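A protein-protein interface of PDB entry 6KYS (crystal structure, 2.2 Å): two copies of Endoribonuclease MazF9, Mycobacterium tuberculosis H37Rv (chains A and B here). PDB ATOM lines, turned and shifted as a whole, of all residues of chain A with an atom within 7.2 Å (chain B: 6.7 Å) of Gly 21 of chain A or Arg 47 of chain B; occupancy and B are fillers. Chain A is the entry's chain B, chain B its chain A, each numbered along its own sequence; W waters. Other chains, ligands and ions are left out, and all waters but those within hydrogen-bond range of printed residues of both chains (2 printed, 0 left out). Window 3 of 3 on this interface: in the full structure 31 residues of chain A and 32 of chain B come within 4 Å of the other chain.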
ATOM      1  N   ALA A  19      22.514  -9.228 -17.607  1.00  0.00           N
ATOM      2  CA  ALA A  19      23.483 -10.164 -17.059  1.00  0.00           C
ATOM      3  C   ALA A  19      22.830 -11.523 -16.859  1.00  0.00           C
ATOM      4  O   ALA A  19      21.604 -11.637 -16.771  1.00  0.00           O
ATOM      5  CB  ALA A  19      24.057  -9.657 -15.728  1.00  0.00           C
ATOM      6  N   ARG A  20      23.666 -12.562 -16.779  1.00  0.00           N
ATOM      7  CA  ARG A  20      23.205 -13.932 -16.601  1.00  0.00           C
ATOM      8  C   ARG A  20      23.913 -14.568 -15.412  1.00  0.00           C
ATOM      9  O   ARG A  20      25.058 -14.235 -15.103  1.00  0.00           O
ATOM     10  CB  ARG A  20      23.446 -14.776 -17.867  1.00  0.00           C
ATOM     11  CG  ARG A  20      22.817 -14.188 -19.130  1.00  0.00           C
ATOM     12  CD  ARG A  20      23.137 -15.012 -20.372  1.00  0.00           C
ATOM     13  NE  ARG A  20      22.696 -16.396 -20.228  1.00  0.00           N
ATOM     14  CZ  ARG A  20      22.844 -17.332 -21.161  1.00  0.00           C
ATOM     15  NH1 ARG A  20      23.425 -17.034 -22.321  1.00  0.00           N
ATOM     16  NH2 ARG A  20      22.412 -18.567 -20.932  1.00  0.00           N
ATOM     17  N   GLY A  21      23.220 -15.485 -14.743  1.00  0.00           N
ATOM     18  CA  GLY A  21      23.835 -16.217 -13.645  1.00  0.00           C
ATOM     19  C   GLY A  21      24.310 -15.305 -12.529  1.00  0.00           C
ATOM     20  O   GLY A  21      23.617 -14.366 -12.124  1.00  0.00           O
ATOM     21  N   SER A  22      25.516 -15.586 -12.020  1.00  0.00           N
ATOM     22  CA  SER A  22      26.128 -14.825 -10.932  1.00  0.00           C
ATOM     23  C   SER A  22      26.805 -13.543 -11.382  1.00  0.00           C
ATOM     24  O   SER A  22      27.441 -12.884 -10.551  1.00  0.00           O
ATOM     25  CB  SER A  22      27.160 -15.671 -10.186  1.00  0.00           C
ATOM     26  OG  SER A  22      26.550 -16.405  -9.150  1.00  0.00           O
ATOM     27  N   GLU A  23      26.702 -13.185 -12.656  1.00  0.00           N
ATOM     28  CA  GLU A  23      27.327 -11.965 -13.136  1.00  0.00           C
ATOM     29  C   GLU A  23      26.795 -10.760 -12.368  1.00  0.00           C
ATOM     30  O   GLU A  23      25.588 -10.640 -12.130  1.00  0.00           O
ATOM     31  CB  GLU A  23      27.086 -11.811 -14.644  1.00  0.00           C
ATOM     32  CG  GLU A  23      27.855 -12.839 -15.482  1.00  0.00           C
ATOM     33  CD  GLU A  23      27.339 -12.998 -16.912  1.00  0.00           C
ATOM     34  OE1 GLU A  23      26.435 -12.238 -17.324  1.00  0.00           O
ATOM     35  OE2 GLU A  23      27.838 -13.908 -17.617  1.00  0.00           O
ATOM     36  N   ALA A  24      27.713  -9.895 -11.935  1.00  0.00           N
ATOM     37  CA  ALA A  24      27.333  -8.604 -11.380  1.00  0.00           C
ATOM     38  C   ALA A  24      26.451  -7.850 -12.369  1.00  0.00           C
ATOM     39  O   ALA A  24      26.761  -7.767 -13.561  1.00  0.00           O
ATOM     40  CB  ALA A  24      28.581  -7.785 -11.051  1.00  0.00           C
ATOM     41  N   ASN A  25      25.351  -7.290 -11.867  1.00  0.00           N
ATOM     42  CA  ASN A  25      24.274  -6.804 -12.719  1.00  0.00           C
ATOM     43  C   ASN A  25      23.902  -5.372 -12.345  1.00  0.00           C
ATOM     44  O   ASN A  25      24.500  -4.759 -11.451  1.00  0.00           O
ATOM     45  CB  ASN A  25      23.055  -7.730 -12.625  1.00  0.00           C
ATOM     46  CG  ASN A  25      22.509  -7.830 -11.216  1.00  0.00           C
ATOM     47  OD1 ASN A  25      22.982  -7.152 -10.300  1.00  0.00           O
ATOM     48  ND2 ASN A  25      21.503  -8.676 -11.032  1.00  0.00           N
ATOM     49  N   THR B  41      35.745 -24.166  -7.977  1.00  0.00           N
ATOM     50  CA  THR B  41      34.651 -23.622  -7.176  1.00  0.00           C
ATOM     51  C   THR B  41      33.418 -23.360  -8.036  1.00  0.00           C
ATOM     52  O   THR B  41      32.296 -23.730  -7.670  1.00  0.00           O
ATOM     53  CB  THR B  41      35.101 -22.338  -6.476  1.00  0.00           C
ATOM     54  OG1 THR B  41      36.260 -22.607  -5.678  1.00  0.00           O
ATOM     55  CG2 THR B  41      33.990 -21.796  -5.578  1.00  0.00           C
ATOM     56  N   ALA B  42      33.615 -22.706  -9.184  1.00  0.00           N
ATOM     57  CA  ALA B  42      32.511 -22.402 -10.088  1.00  0.00           C
ATOM     58  C   ALA B  42      31.795 -23.669 -10.539  1.00  0.00           C
ATOM     59  O   ALA B  42      30.564 -23.690 -10.641  1.00  0.00           O
ATOM     60  CB  ALA B  42      33.032 -21.615 -11.291  1.00  0.00           C
ATOM     61  N   THR B  43      32.548 -24.743 -10.794  1.00  0.00           N
ATOM     62  CA  THR B  43      31.913 -26.000 -11.180  1.00  0.00           C
ATOM     63  C   THR B  43      31.219 -26.654 -10.000  1.00  0.00           C
ATOM     64  O   THR B  43      30.282 -27.437 -10.192  1.00  0.00           O
ATOM     65  CB  THR B  43      32.934 -26.985 -11.757  1.00  0.00           C
ATOM     66  OG1 THR B  43      33.847 -27.362 -10.726  1.00  0.00           O
ATOM     67  CG2 THR B  43      33.706 -26.387 -12.900  1.00  0.00           C
ATOM     68  N   ARG B  44      31.700 -26.378  -8.784  1.00  0.00           N
ATOM     69  CA  ARG B  44      31.119 -26.914  -7.560  1.00  0.00           C
ATOM     70  C   ARG B  44      29.669 -26.473  -7.413  1.00  0.00           C
ATOM     71  O   ARG B  44      28.755 -27.267  -7.650  1.00  0.00           O
ATOM     72  CB  ARG B  44      31.930 -26.476  -6.337  1.00  0.00           C
ATOM     73  N   LEU B  45      29.458 -25.208  -7.032  1.00  0.00           N
ATOM     74  CA  LEU B  45      28.108 -24.659  -6.913  1.00  0.00           C
ATOM     75  C   LEU B  45      27.266 -24.892  -8.166  1.00  0.00           C
ATOM     76  O   LEU B  45      26.040 -25.028  -8.074  1.00  0.00           O
ATOM     77  CB  LEU B  45      28.177 -23.160  -6.624  1.00  0.00           C
ATOM     78  N   GLY B  46      27.901 -24.904  -9.346  1.00  0.00           N
ATOM     79  CA  GLY B  46      27.212 -25.007 -10.626  1.00  0.00           C
ATOM     80  C   GLY B  46      27.125 -23.650 -11.299  1.00  0.00           C
ATOM     81  O   GLY B  46      27.467 -23.495 -12.477  1.00  0.00           O
ATOM     82  N   ARG B  47      26.672 -22.654 -10.530  1.00  0.00           N
ATOM     83  CA  ARG B  47      26.712 -21.256 -10.937  1.00  0.00           C
ATOM     84  C   ARG B  47      28.166 -20.784 -10.836  1.00  0.00           C
ATOM     85  O   ARG B  47      29.069 -21.414 -11.402  1.00  0.00           O
ATOM     86  CB  ARG B  47      25.736 -20.414 -10.086  1.00  0.00           C
ATOM     87  CG  ARG B  47      25.687 -18.940 -10.456  1.00  0.00           C
ATOM     88  CD  ARG B  47      24.311 -18.384 -10.680  1.00  0.00           C
ATOM     89  NE  ARG B  47      23.468 -18.452  -9.494  1.00  0.00           N
ATOM     90  CZ  ARG B  47      22.305 -17.821  -9.357  1.00  0.00           C
ATOM     91  NH1 ARG B  47      21.854 -17.041 -10.329  1.00  0.00           N
ATOM     92  NH2 ARG B  47      21.620 -17.953  -8.225  1.00  0.00           N
ATOM     93  N   GLY B  48      28.417 -19.700 -10.110  1.00  0.00           N
ATOM     94  CA  GLY B  48      29.718 -19.067 -10.132  1.00  0.00           C
ATOM     95  C   GLY B  48      30.123 -18.554 -11.501  1.00  0.00           C
ATOM     96  O   GLY B  48      29.429 -18.755 -12.505  1.00  0.00           O
ATOM     97  N   VAL B  49      31.267 -17.890 -11.548  1.00  0.00           N
ATOM     98  CA  VAL B  49      31.745 -17.212 -12.738  1.00  0.00           C
ATOM     99  C   VAL B  49      33.134 -17.752 -13.036  1.00  0.00           C
ATOM    100  O   VAL B  49      33.806 -18.268 -12.139  1.00  0.00           O
ATOM    101  CB  VAL B  49      31.758 -15.685 -12.515  1.00  0.00           C
ATOM    102  CG1 VAL B  49      30.334 -15.174 -12.400  1.00  0.00           C
ATOM    103  CG2 VAL B  49      32.501 -15.361 -11.228  1.00  0.00           C
ATOM    104  N   ILE B  50      33.535 -17.685 -14.300  1.00  0.00           N
ATOM    105  CA  ILE B  50      34.890 -17.998 -14.732  1.00  0.00           C
ATOM    106  C   ILE B  50      35.321 -16.868 -15.653  1.00  0.00           C
ATOM    107  O   ILE B  50      34.486 -16.229 -16.297  1.00  0.00           O
ATOM    108  CB  ILE B  50      34.970 -19.361 -15.456  1.00  0.00           C
ATOM    109  CG1 ILE B  50      33.953 -19.407 -16.603  1.00  0.00           C
ATOM    110  CG2 ILE B  50      34.735 -20.507 -14.483  1.00  0.00           C
ATOM    111  CD1 ILE B  50      34.422 -20.175 -17.820  1.00  0.00           C
ATOM    112  N   ALA B  91      29.172 -16.101 -16.491  1.00  0.00           N
ATOM    113  CA  ALA B  91      28.487 -17.223 -15.864  1.00  0.00           C
ATOM    114  C   ALA B  91      28.842 -18.510 -16.594  1.00  0.00           C
ATOM    115  O   ALA B  91      29.008 -18.520 -17.817  1.00  0.00           O
ATOM    116  CB  ALA B  91      26.973 -17.003 -15.893  1.00  0.00           C
ATOM    117  N   THR B  92      28.963 -19.604 -15.835  1.00  0.00           N
ATOM    118  CA  THR B  92      29.296 -20.892 -16.434  1.00  0.00           C
ATOM    119  C   THR B  92      28.271 -21.326 -17.475  1.00  0.00           C
ATOM    120  O   THR B  92      28.602 -22.110 -18.371  1.00  0.00           O
ATOM    121  CB  THR B  92      29.415 -21.971 -15.351  1.00  0.00           C
ATOM    122  OG1 THR B  92      28.219 -21.992 -14.566  1.00  0.00           O
ATOM    123  CG2 THR B  92      30.607 -21.698 -14.436  1.00  0.00           C
ATOM    124  N   GLU B  93      27.037 -20.832 -17.385  1.00  0.00           N
ATOM    125  CA  GLU B  93      26.018 -21.201 -18.357  1.00  0.00           C
ATOM    126  C   GLU B  93      26.271 -20.610 -19.738  1.00  0.00           C
ATOM    127  O   GLU B  93      25.601 -21.014 -20.692  1.00  0.00           O
ATOM    128  CB  GLU B  93      24.638 -20.772 -17.853  1.00  0.00           C
ATOM    129  CG  GLU B  93      24.450 -19.276 -17.796  1.00  0.00           C
ATOM    130  CD  GLU B  93      23.164 -18.881 -17.106  1.00  0.00           C
ATOM    131  OE1 GLU B  93      22.290 -18.285 -17.769  1.00  0.00           O
ATOM    132  OE2 GLU B  93      23.025 -19.170 -15.899  1.00  0.00           O
HETATM  133  O   HOH W   1      20.649 -16.446 -16.064  1.00  0.00           O
HETATM  134  O   HOH W   2      26.927 -17.858 -12.952  1.00  0.00           O
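Printed residues of chain B within 4 Å of Arg 20 of chain A: Ala 91 and Glu 93. Of chain B, only Arg 47 (3.6 Å), Ala 91 (3.9 Å) and Glu 93 (3.8 Å) come within 4 Å of Gly 21 of chain A. Of the printed residues of chain B, Ser 22 of chain A touches Arg 47 (3.0 Å), Gly 48 (3.9 Å) and Val 49 (3.9 Å). Printed residues of chain B within 4 Å of Glu 23 of chain A: Ala 91. Ala 24 of chain A touches none of the printed residues of chain B. No residue of chain A comes within 4 Å of Gly 46 of chain B. Of chain A, only Gly 21 (3.6 Å) and Ser 22 (3.0 Å) come within 4 Å of Arg 47 of chain B. Of the printed residues of chain A, Ala 91 of chain B touches Arg 20, Gly 21 and Glu 23. Of the printed residues of chain A, Glu 93 of chain B touches Arg 20 and Gly 21.
The backbone carbonyl oxygen (O) of Arg 47 of chain B lies within hydrogen-bond range of the side-chain hydroxyl (OG1) of Thr 92 of chain B (3.3 Å). N of Thr 92 of chain B sits at hydrogen-bond distance from O of Gly 48 of chain B. N of Arg 20 of chain A sits at hydrogen-bond distance from OE1 of Glu 23 of chain A, at 2.8 Å.
Of the 7 printed residues of chain A, 4 touch a printed residue of chain B. Printed residues of chain A that touch a printed residue of chain B: Arg 20, Gly 21, Ser 22 and Glu 23. Along chain A the printed residues that touch a printed residue of chain B span positions 20 to 23.
No position is printed for both chains. Of the 9 pairs that touch across the chains among the printed residues, none has its exchanged pair printed and touching as well.
The backbone NH of Ala 91 of chain B lies within hydrogen-bond range of the side-chain carboxylate of Glu 23 of chain A, 2.8 Å away. NE of Arg 20 of chain A is in salt-bridge range of OE1 of Glu 93 of chain B (3.1 Å).
Arg 20 of chain A touches Ala 91 of chain B. Arg 47 of chain B touches Gly 21 of chain A (CD to C, 3.6 Å). CB of Ala 91 of chain B touches CA of Gly 21 of chain A, 3.9 Å away. Gly 21 of chain A touches Glu 93 of chain B. Arg 47 of chain B touches Ser 22 of chain A. OG of Ser 22 of chain A touches N of Gly 48 of chain B, 3.9 Å away. Val 49 of chain B touches Ser 22 of chain A (CG1 to CB, 3.9 Å).
Water W2 bridges O of Gly 48 of chain B and N of Ser 22 of chain A. Water W1 lies within hydrogen-bond range of the side-chain carboxylate (OE1) of Glu 93 of chain B (3.0 Å) and the backbone NH (N) of Gly 21 of chain A (3.0 Å).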
